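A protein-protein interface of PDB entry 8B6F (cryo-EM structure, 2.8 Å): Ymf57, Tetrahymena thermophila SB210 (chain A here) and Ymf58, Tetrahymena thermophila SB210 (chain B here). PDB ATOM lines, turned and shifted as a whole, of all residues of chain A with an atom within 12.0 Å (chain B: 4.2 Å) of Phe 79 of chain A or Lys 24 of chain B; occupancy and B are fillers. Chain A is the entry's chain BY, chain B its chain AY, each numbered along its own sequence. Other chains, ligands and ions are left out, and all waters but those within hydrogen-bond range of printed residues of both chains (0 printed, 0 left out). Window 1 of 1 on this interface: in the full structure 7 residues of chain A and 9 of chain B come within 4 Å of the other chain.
The side-chain amino group (NZ) of Lys 24 of chain B sits at hydrogen-bond distance from the backbone carbonyl oxygen (O) of Lys 22 of chain B (3.1 Å).
The backbone NH of Thr 90 of chain B is in hydrogen-bond range of the backbone carbonyl oxygen of Lys 24 of chain B, 2.9 Å away.
Among the printed residues, merely in contact across the chains: Phe 79 of chain A with Lys 24 of chain B, Glu 75 of chain A with Thr 90 of chain B, Leu 83 of chain A with Val 20 of chain B, Phe 79 of chain A with Val 20 of chain B, Phe 79 of chain A with Leu 19 of chain B, Phe 79 of chain A with Ile 29 of chain B and Ser 76 of chain A with Lys 24 of chain B.
Phe 79 of chain A touches just these residues of chain B: Leu 19, Val 20, Lys 24 and Ile 29.
Of the printed residues of chain A, Lys 24 of chain B touches Ser 76 (3.96 Å) and Phe 79 (3.3 Å).
Of chain A, only Phe 79 comes within 4 Å of Leu 19 of chain B.
No residue of chain A comes within 4 Å of Asn 89 of chain B.
Thr 90 of chain B touches just one residue of chain A: Glu 75 (3.5 Å).
Printed residues of chain B within 4 Å of Leu 83 of chain A: Val 20.
Printed residues of chain B within 4 Å of Ser 76 of chain A: Lys 24.
Of the printed residues of chain B, Glu 75 of chain A touches Thr 90 (3.5 Å).
The nearest printed residue of chain B that does not touch Phe 79 of chain A is Thr 90 of chain B (6.5 Å).
The nearest residue of chain A that does not touch Lys 24 of chain B is Glu 75 of chain A (4.5 Å).
Of the 11 printed residues of chain B, 5 touch a printed residue of chain A.
Hydrophobic or aromatic side chains of chain B within 4 Å of the printed part of chain A: Leu 19, Val 20 and Ile 29.
Hydrophobic or aromatic side chains of chain A that line the printed part of chain B: Phe 79 and Leu 83.
Among the printed residues, 7 pairs touch across the chains.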
ATOM      1  N   PHE A  70      -8.936  10.802   8.586  1.00  0.00           N
ATOM      2  CA  PHE A  70      -8.555  12.199   8.718  1.00  0.00           C
ATOM      3  C   PHE A  70      -9.659  13.089   8.160  1.00  0.00           C
ATOM      4  O   PHE A  70     -10.117  12.888   7.031  1.00  0.00           O
ATOM      5  CB  PHE A  70      -7.241  12.473   7.989  1.00  0.00           C
ATOM      6  CG  PHE A  70      -6.025  12.028   8.743  1.00  0.00           C
ATOM      7  CD1 PHE A  70      -5.394  12.885   9.628  1.00  0.00           C
ATOM      8  CD2 PHE A  70      -5.507  10.757   8.563  1.00  0.00           C
ATOM      9  CE1 PHE A  70      -4.275  12.481  10.325  1.00  0.00           C
ATOM     10  CE2 PHE A  70      -4.388  10.348   9.256  1.00  0.00           C
ATOM     11  CZ  PHE A  70      -3.770  11.212  10.139  1.00  0.00           C
ATOM     12  N   ASN A  72      -9.474  16.293   7.332  1.00  0.00           N
ATOM     13  CA  ASN A  72      -8.941  17.145   6.277  1.00  0.00           C
ATOM     14  C   ASN A  72      -7.944  16.366   5.433  1.00  0.00           C
ATOM     15  O   ASN A  72      -7.015  15.754   5.970  1.00  0.00           O
ATOM     16  CB  ASN A  72      -8.270  18.387   6.867  1.00  0.00           C
ATOM     17  CG  ASN A  72      -9.230  19.244   7.661  1.00  0.00           C
ATOM     18  OD1 ASN A  72      -9.038  19.468   8.856  1.00  0.00           O
ATOM     19  ND2 ASN A  72     -10.272  19.733   6.999  1.00  0.00           N
ATOM     20  N   LEU A  73      -8.133  16.399   4.119  1.00  0.00           N
ATOM     21  CA  LEU A  73      -7.220  15.719   3.214  1.00  0.00           C
ATOM     22  C   LEU A  73      -5.882  16.446   3.162  1.00  0.00           C
ATOM     23  O   LEU A  73      -5.806  17.668   3.308  1.00  0.00           O
ATOM     24  CB  LEU A  73      -7.825  15.634   1.812  1.00  0.00           C
ATOM     25  CG  LEU A  73      -6.942  15.012   0.726  1.00  0.00           C
ATOM     26  CD1 LEU A  73      -6.670  13.552   1.028  1.00  0.00           C
ATOM     27  CD2 LEU A  73      -7.581  15.162  -0.638  1.00  0.00           C
ATOM     28  N   VAL A  74      -4.817  15.674   2.948  1.00  0.00           N
ATOM     29  CA  VAL A  74      -3.480  16.210   2.753  1.00  0.00           C
ATOM     30  C   VAL A  74      -2.893  15.583   1.497  1.00  0.00           C
ATOM     31  O   VAL A  74      -3.319  14.520   1.044  1.00  0.00           O
ATOM     32  CB  VAL A  74      -2.558  15.967   3.969  1.00  0.00           C
ATOM     33  CG1 VAL A  74      -3.156  16.582   5.217  1.00  0.00           C
ATOM     34  CG2 VAL A  74      -2.309  14.487   4.176  1.00  0.00           C
ATOM     35  N   GLU A  75      -1.891  16.263   0.936  1.00  0.00           N
ATOM     36  CA  GLU A  75      -1.338  15.845  -0.348  1.00  0.00           C
ATOM     37  C   GLU A  75      -0.675  14.478  -0.247  1.00  0.00           C
ATOM     38  O   GLU A  75      -0.794  13.655  -1.162  1.00  0.00           O
ATOM     39  CB  GLU A  75      -0.347  16.889  -0.859  1.00  0.00           C
ATOM     40  CG  GLU A  75      -0.974  18.238  -1.199  1.00  0.00           C
ATOM     41  CD  GLU A  75      -1.330  19.063   0.021  1.00  0.00           C
ATOM     42  OE1 GLU A  75      -0.982  18.649   1.147  1.00  0.00           O
ATOM     43  OE2 GLU A  75      -1.962  20.127  -0.145  1.00  0.00           O
ATOM     44  N   SER A  76       0.026  14.215   0.855  1.00  0.00           N
ATOM     45  CA  SER A  76       0.657  12.910   1.031  1.00  0.00           C
ATOM     46  C   SER A  76      -0.381  11.796   0.997  1.00  0.00           C
ATOM     47  O   SER A  76      -0.199  10.782   0.314  1.00  0.00           O
ATOM     48  CB  SER A  76       1.429  12.882   2.349  1.00  0.00           C
ATOM     49  OG  SER A  76       2.342  13.962   2.427  1.00  0.00           O
ATOM     50  N   LYS A  77      -1.478  11.967   1.734  1.00  0.00           N
ATOM     51  CA  LYS A  77      -2.538  10.964   1.730  1.00  0.00           C
ATOM     52  C   LYS A  77      -3.152  10.824   0.345  1.00  0.00           C
ATOM     53  O   LYS A  77      -3.437   9.709  -0.105  1.00  0.00           O
ATOM     54  CB  LYS A  77      -3.611  11.337   2.752  1.00  0.00           C
ATOM     55  CG  LYS A  77      -3.163  11.213   4.201  1.00  0.00           C
ATOM     56  CD  LYS A  77      -3.012   9.760   4.621  1.00  0.00           C
ATOM     57  CE  LYS A  77      -2.678   9.651   6.101  1.00  0.00           C
ATOM     58  NZ  LYS A  77      -2.607   8.234   6.551  1.00  0.00           N
ATOM     59  N   TYR A  78      -3.366  11.944  -0.345  1.00  0.00           N
ATOM     60  CA  TYR A  78      -3.944  11.891  -1.683  1.00  0.00           C
ATOM     61  C   TYR A  78      -3.090  11.037  -2.613  1.00  0.00           C
ATOM     62  O   TYR A  78      -3.592  10.109  -3.257  1.00  0.00           O
ATOM     63  CB  TYR A  78      -4.094  13.315  -2.224  1.00  0.00           C
ATOM     64  CG  TYR A  78      -4.447  13.408  -3.687  1.00  0.00           C
ATOM     65  CD1 TYR A  78      -5.727  13.111  -4.137  1.00  0.00           C
ATOM     66  CD2 TYR A  78      -3.510  13.834  -4.617  1.00  0.00           C
ATOM     67  CE1 TYR A  78      -6.054  13.209  -5.474  1.00  0.00           C
ATOM     68  CE2 TYR A  78      -3.827  13.936  -5.954  1.00  0.00           C
ATOM     69  CZ  TYR A  78      -5.101  13.624  -6.376  1.00  0.00           C
ATOM     70  OH  TYR A  78      -5.421  13.723  -7.708  1.00  0.00           O
ATOM     71  N   PHE A  79      -1.794  11.339  -2.702  1.00  0.00           N
ATOM     72  CA  PHE A  79      -0.922  10.587  -3.599  1.00  0.00           C
ATOM     73  C   PHE A  79      -0.794   9.131  -3.168  1.00  0.00           C
ATOM     74  O   PHE A  79      -0.809   8.225  -4.007  1.00  0.00           O
ATOM     75  CB  PHE A  79       0.454  11.248  -3.671  1.00  0.00           C
ATOM     76  CG  PHE A  79       0.477  12.494  -4.504  1.00  0.00           C
ATOM     77  CD1 PHE A  79       0.478  12.413  -5.886  1.00  0.00           C
ATOM     78  CD2 PHE A  79       0.496  13.742  -3.912  1.00  0.00           C
ATOM     79  CE1 PHE A  79       0.498  13.553  -6.659  1.00  0.00           C
ATOM     80  CE2 PHE A  79       0.517  14.887  -4.682  1.00  0.00           C
ATOM     81  CZ  PHE A  79       0.516  14.791  -6.057  1.00  0.00           C
ATOM     82  N   LEU A  80      -0.669   8.889  -1.861  1.00  0.00           N
ATOM     83  CA  LEU A  80      -0.508   7.522  -1.373  1.00  0.00           C
ATOM     84  C   LEU A  80      -1.750   6.686  -1.646  1.00  0.00           C
ATOM     85  O   LEU A  80      -1.643   5.505  -1.994  1.00  0.00           O
ATOM     86  CB  LEU A  80      -0.186   7.529   0.122  1.00  0.00           C
ATOM     87  CG  LEU A  80       0.127   6.162   0.740  1.00  0.00           C
ATOM     88  CD1 LEU A  80       1.307   5.495   0.044  1.00  0.00           C
ATOM     89  CD2 LEU A  80       0.397   6.296   2.229  1.00  0.00           C
ATOM     90  N   GLN A  81      -2.936   7.272  -1.485  1.00  0.00           N
ATOM     91  CA  GLN A  81      -4.160   6.542  -1.794  1.00  0.00           C
ATOM     92  C   GLN A  81      -4.247   6.217  -3.279  1.00  0.00           C
ATOM     93  O   GLN A  81      -4.658   5.114  -3.655  1.00  0.00           O
ATOM     94  CB  GLN A  81      -5.382   7.346  -1.351  1.00  0.00           C
ATOM     95  CG  GLN A  81      -5.553   7.416   0.153  1.00  0.00           C
ATOM     96  CD  GLN A  81      -6.756   8.239   0.559  1.00  0.00           C
ATOM     97  OE1 GLN A  81      -7.582   8.604  -0.276  1.00  0.00           O
ATOM     98  NE2 GLN A  81      -6.861   8.538   1.848  1.00  0.00           N
ATOM     99  N   ILE A  82      -3.877   7.164  -4.142  1.00  0.00           N
ATOM    100  CA  ILE A  82      -3.902   6.895  -5.577  1.00  0.00           C
ATOM    101  C   ILE A  82      -2.965   5.742  -5.912  1.00  0.00           C
ATOM    102  O   ILE A  82      -3.328   4.817  -6.646  1.00  0.00           O
ATOM    103  CB  ILE A  82      -3.546   8.170  -6.366  1.00  0.00           C
ATOM    104  CG1 ILE A  82      -4.771   9.084  -6.450  1.00  0.00           C
ATOM    105  CG2 ILE A  82      -3.029   7.830  -7.765  1.00  0.00           C
ATOM    106  CD1 ILE A  82      -4.504  10.432  -7.075  1.00  0.00           C
ATOM    107  N   LEU A  83      -1.742   5.780  -5.377  1.00  0.00           N
ATOM    108  CA  LEU A  83      -0.785   4.717  -5.667  1.00  0.00           C
ATOM    109  C   LEU A  83      -1.255   3.388  -5.097  1.00  0.00           C
ATOM    110  O   LEU A  83      -1.103   2.343  -5.740  1.00  0.00           O
ATOM    111  CB  LEU A  83       0.594   5.075  -5.116  1.00  0.00           C
ATOM    112  CG  LEU A  83       1.691   4.041  -5.388  1.00  0.00           C
ATOM    113  CD1 LEU A  83       1.919   3.877  -6.882  1.00  0.00           C
ATOM    114  CD2 LEU A  83       2.985   4.422  -4.693  1.00  0.00           C
ATOM    115  N   THR A  84      -1.821   3.404  -3.891  1.00  0.00           N
ATOM    116  CA  THR A  84      -2.311   2.168  -3.293  1.00  0.00           C
ATOM    117  C   THR A  84      -3.403   1.551  -4.153  1.00  0.00           C
ATOM    118  O   THR A  84      -3.406   0.341  -4.403  1.00  0.00           O
ATOM    119  CB  THR A  84      -2.828   2.438  -1.878  1.00  0.00           C
ATOM    120  OG1 THR A  84      -1.795   3.047  -1.094  1.00  0.00           O
ATOM    121  CG2 THR A  84      -3.265   1.146  -1.208  1.00  0.00           C
ATOM    122  N   LEU A  85      -4.352   2.369  -4.609  1.00  0.00           N
ATOM    123  CA  LEU A  85      -5.375   1.864  -5.514  1.00  0.00           C
ATOM    124  C   LEU A  85      -4.741   1.265  -6.763  1.00  0.00           C
ATOM    125  O   LEU A  85      -5.042   0.127  -7.142  1.00  0.00           O
ATOM    126  CB  LEU A  85      -6.347   2.986  -5.879  1.00  0.00           C
ATOM    127  CG  LEU A  85      -7.443   2.624  -6.882  1.00  0.00           C
ATOM    128  CD1 LEU A  85      -8.303   1.478  -6.369  1.00  0.00           C
ATOM    129  CD2 LEU A  85      -8.300   3.838  -7.198  1.00  0.00           C
ATOM    130  N   ILE A  86      -3.874   2.030  -7.430  1.00  0.00           N
ATOM    131  CA  ILE A  86      -3.296   1.576  -8.693  1.00  0.00           C
ATOM    132  C   ILE A  86      -2.613   0.227  -8.517  1.00  0.00           C
ATOM    133  O   ILE A  86      -2.829  -0.706  -9.298  1.00  0.00           O
ATOM    134  CB  ILE A  86      -2.314   2.630  -9.241  1.00  0.00           C
ATOM    135  CG1 ILE A  86      -3.076   3.855  -9.750  1.00  0.00           C
ATOM    136  CG2 ILE A  86      -1.439   2.040 -10.353  1.00  0.00           C
ATOM    137  CD1 ILE A  86      -2.191   5.025 -10.130  1.00  0.00           C
ATOM    138  N   LEU A  87      -1.774   0.104  -7.485  1.00  0.00           N
ATOM    139  CA  LEU A  87      -0.982  -1.111  -7.325  1.00  0.00           C
ATOM    140  C   LEU A  87      -1.832  -2.285  -6.860  1.00  0.00           C
ATOM    141  O   LEU A  87      -1.725  -3.391  -7.402  1.00  0.00           O
ATOM    142  CB  LEU A  87       0.166  -0.861  -6.344  1.00  0.00           C
ATOM    143  CG  LEU A  87       1.293   0.054  -6.831  1.00  0.00           C
ATOM    144  CD1 LEU A  87       2.278   0.320  -5.708  1.00  0.00           C
ATOM    145  CD2 LEU A  87       2.009  -0.545  -8.030  1.00  0.00           C
ATOM    146  N   TYR A  88      -2.673  -2.074  -5.851  1.00  0.00           N
ATOM    147  CA  TYR A  88      -3.307  -3.205  -5.186  1.00  0.00           C
ATOM    148  C   TYR A  88      -4.612  -3.644  -5.828  1.00  0.00           C
ATOM    149  O   TYR A  88      -5.005  -4.802  -5.652  1.00  0.00           O
ATOM    150  CB  TYR A  88      -3.525  -2.885  -3.706  1.00  0.00           C
ATOM    151  CG  TYR A  88      -2.221  -2.905  -2.951  1.00  0.00           C
ATOM    152  CD1 TYR A  88      -1.655  -4.106  -2.547  1.00  0.00           C
ATOM    153  CD2 TYR A  88      -1.533  -1.732  -2.678  1.00  0.00           C
ATOM    154  CE1 TYR A  88      -0.453  -4.140  -1.878  1.00  0.00           C
ATOM    155  CE2 TYR A  88      -0.330  -1.754  -2.007  1.00  0.00           C
ATOM    156  CZ  TYR A  88       0.205  -2.961  -1.608  1.00  0.00           C
ATOM    157  OH  TYR A  88       1.403  -2.989  -0.938  1.00  0.00           O
ATOM    158  N   LEU B  19       7.389   9.386  -8.337  1.00  0.00           N
ATOM    159  CA  LEU B  19       6.636  10.616  -8.125  1.00  0.00           C
ATOM    160  C   LEU B  19       5.867  10.560  -6.813  1.00  0.00           C
ATOM    161  O   LEU B  19       5.891  11.510  -6.023  1.00  0.00           O
ATOM    162  CB  LEU B  19       5.691  10.852  -9.306  1.00  0.00           C
ATOM    163  CG  LEU B  19       4.760  12.069  -9.280  1.00  0.00           C
ATOM    164  CD1 LEU B  19       4.367  12.439 -10.694  1.00  0.00           C
ATOM    165  CD2 LEU B  19       3.500  11.822  -8.463  1.00  0.00           C
ATOM    166  N   VAL B  20       5.178   9.448  -6.563  1.00  0.00           N
ATOM    167  CA  VAL B  20       4.414   9.309  -5.330  1.00  0.00           C
ATOM    168  C   VAL B  20       5.350   9.208  -4.131  1.00  0.00           C
ATOM    169  O   VAL B  20       5.044   9.711  -3.044  1.00  0.00           O
ATOM    170  CB  VAL B  20       3.474   8.095  -5.424  1.00  0.00           C
ATOM    171  CG1 VAL B  20       2.744   7.875  -4.106  1.00  0.00           C
ATOM    172  CG2 VAL B  20       2.490   8.276  -6.569  1.00  0.00           C
ATOM    173  N   LYS B  22       8.593  10.337  -3.535  1.00  0.00           N
ATOM    174  CA  LYS B  22       9.414  11.450  -3.093  1.00  0.00           C
ATOM    175  C   LYS B  22       8.593  12.404  -2.227  1.00  0.00           C
ATOM    176  O   LYS B  22       7.376  12.519  -2.397  1.00  0.00           O
ATOM    177  CB  LYS B  22       9.993  12.196  -4.290  1.00  0.00           C
ATOM    178  CG  LYS B  22      11.048  11.406  -5.048  1.00  0.00           C
ATOM    179  CD  LYS B  22      11.750  12.248  -6.106  1.00  0.00           C
ATOM    180  CE  LYS B  22      12.558  13.384  -5.498  1.00  0.00           C
ATOM    181  NZ  LYS B  22      13.474  12.920  -4.421  1.00  0.00           N
ATOM    182  N   PRO B  23       9.233  13.100  -1.287  1.00  0.00           N
ATOM    183  CA  PRO B  23       8.487  14.039  -0.441  1.00  0.00           C
ATOM    184  C   PRO B  23       7.765  15.075  -1.287  1.00  0.00           C
ATOM    185  O   PRO B  23       8.287  15.559  -2.293  1.00  0.00           O
ATOM    186  CB  PRO B  23       9.571  14.675   0.437  1.00  0.00           C
ATOM    187  CG  PRO B  23      10.852  14.407  -0.265  1.00  0.00           C
ATOM    188  CD  PRO B  23      10.670  13.106  -0.972  1.00  0.00           C
ATOM    189  N   LYS B  24       6.553  15.415  -0.866  1.00  0.00           N
ATOM    190  CA  LYS B  24       5.646  16.214  -1.684  1.00  0.00           C
ATOM    191  C   LYS B  24       6.087  17.670  -1.649  1.00  0.00           C
ATOM    192  O   LYS B  24       5.628  18.467  -0.830  1.00  0.00           O
ATOM    193  CB  LYS B  24       4.209  16.049  -1.206  1.00  0.00           C
ATOM    194  CG  LYS B  24       3.719  14.609  -1.234  1.00  0.00           C
ATOM    195  CD  LYS B  24       3.732  14.034  -2.645  1.00  0.00           C
ATOM    196  CE  LYS B  24       3.355  12.566  -2.643  1.00  0.00           C
ATOM    197  NZ  LYS B  24       4.406  11.713  -2.026  1.00  0.00           N
ATOM    198  N   ASN B  25       6.995  18.016  -2.555  1.00  0.00           N
ATOM    199  CA  ASN B  25       7.353  19.396  -2.845  1.00  0.00           C
ATOM    200  C   ASN B  25       6.874  19.701  -4.258  1.00  0.00           C
ATOM    201  O   ASN B  25       7.246  18.998  -5.202  1.00  0.00           O
ATOM    202  CB  ASN B  25       8.859  19.609  -2.715  1.00  0.00           C
ATOM    203  CG  ASN B  25       9.257  21.062  -2.842  1.00  0.00           C
ATOM    204  OD1 ASN B  25       8.748  21.786  -3.694  1.00  0.00           O
ATOM    205  ND2 ASN B  25      10.170  21.499  -1.987  1.00  0.00           N
ATOM    206  N   PHE B  26       6.061  20.750  -4.400  1.00  0.00           N
ATOM    207  CA  PHE B  26       5.360  20.976  -5.661  1.00  0.00           C
ATOM    208  C   PHE B  26       6.320  20.991  -6.841  1.00  0.00           C
ATOM    209  O   PHE B  26       6.011  20.453  -7.909  1.00  0.00           O
ATOM    210  CB  PHE B  26       4.577  22.286  -5.597  1.00  0.00           C
ATOM    211  CG  PHE B  26       3.610  22.463  -6.731  1.00  0.00           C
ATOM    212  CD1 PHE B  26       4.006  23.070  -7.910  1.00  0.00           C
ATOM    213  CD2 PHE B  26       2.305  22.016  -6.619  1.00  0.00           C
ATOM    214  CE1 PHE B  26       3.117  23.230  -8.955  1.00  0.00           C
ATOM    215  CE2 PHE B  26       1.412  22.174  -7.660  1.00  0.00           C
ATOM    216  CZ  PHE B  26       1.819  22.782  -8.830  1.00  0.00           C
ATOM    217  N   ILE B  29       7.382  17.426  -7.650  1.00  0.00           N
ATOM    218  CA  ILE B  29       6.293  16.683  -8.276  1.00  0.00           C
ATOM    219  C   ILE B  29       6.110  17.141  -9.716  1.00  0.00           C
ATOM    220  O   ILE B  29       5.799  16.338 -10.604  1.00  0.00           O
ATOM    221  CB  ILE B  29       4.989  16.836  -7.471  1.00  0.00           C
ATOM    222  CG1 ILE B  29       5.232  16.554  -5.986  1.00  0.00           C
ATOM    223  CG2 ILE B  29       3.967  15.836  -7.982  1.00  0.00           C
ATOM    224  CD1 ILE B  29       3.994  16.679  -5.111  1.00  0.00           C
ATOM    225  N   LEU B  88       6.103  25.180  -0.069  1.00  0.00           N
ATOM    226  CA  LEU B  88       6.190  24.242  -1.180  1.00  0.00           C
ATOM    227  C   LEU B  88       6.221  22.806  -0.683  1.00  0.00           C
ATOM    228  O   LEU B  88       5.672  21.910  -1.334  1.00  0.00           O
ATOM    229  CB  LEU B  88       7.424  24.545  -2.030  1.00  0.00           C
ATOM    230  CG  LEU B  88       7.378  25.854  -2.821  1.00  0.00           C
ATOM    231  CD1 LEU B  88       8.721  26.131  -3.469  1.00  0.00           C
ATOM    232  CD2 LEU B  88       6.282  25.824  -3.874  1.00  0.00           C
ATOM    233  N   ASN B  89       6.853  22.567   0.463  1.00  0.00           N
ATOM    234  CA  ASN B  89       6.806  21.261   1.115  1.00  0.00           C
ATOM    235  C   ASN B  89       5.432  21.122   1.754  1.00  0.00           C
ATOM    236  O   ASN B  89       5.192  21.615   2.856  1.00  0.00           O
ATOM    237  CB  ASN B  89       7.920  21.134   2.146  1.00  0.00           C
ATOM    238  CG  ASN B  89       9.285  21.426   1.563  1.00  0.00           C
ATOM    239  OD1 ASN B  89       9.862  20.600   0.859  1.00  0.00           O
ATOM    240  ND2 ASN B  89       9.817  22.605   1.864  1.00  0.00           N
ATOM    241  N   THR B  90       4.522  20.440   1.057  1.00  0.00           N
ATOM    242  CA  THR B  90       3.136  20.392   1.507  1.00  0.00           C
ATOM    243  C   THR B  90       3.011  19.774   2.891  1.00  0.00           C
ATOM    244  O   THR B  90       2.086  20.109   3.639  1.00  0.00           O
ATOM    245  CB  THR B  90       2.284  19.612   0.506  1.00  0.00           C
ATOM    246  OG1 THR B  90       2.744  18.257   0.433  1.00  0.00           O
ATOM    247  CG2 THR B  90       2.362  20.247  -0.875  1.00  0.00           C
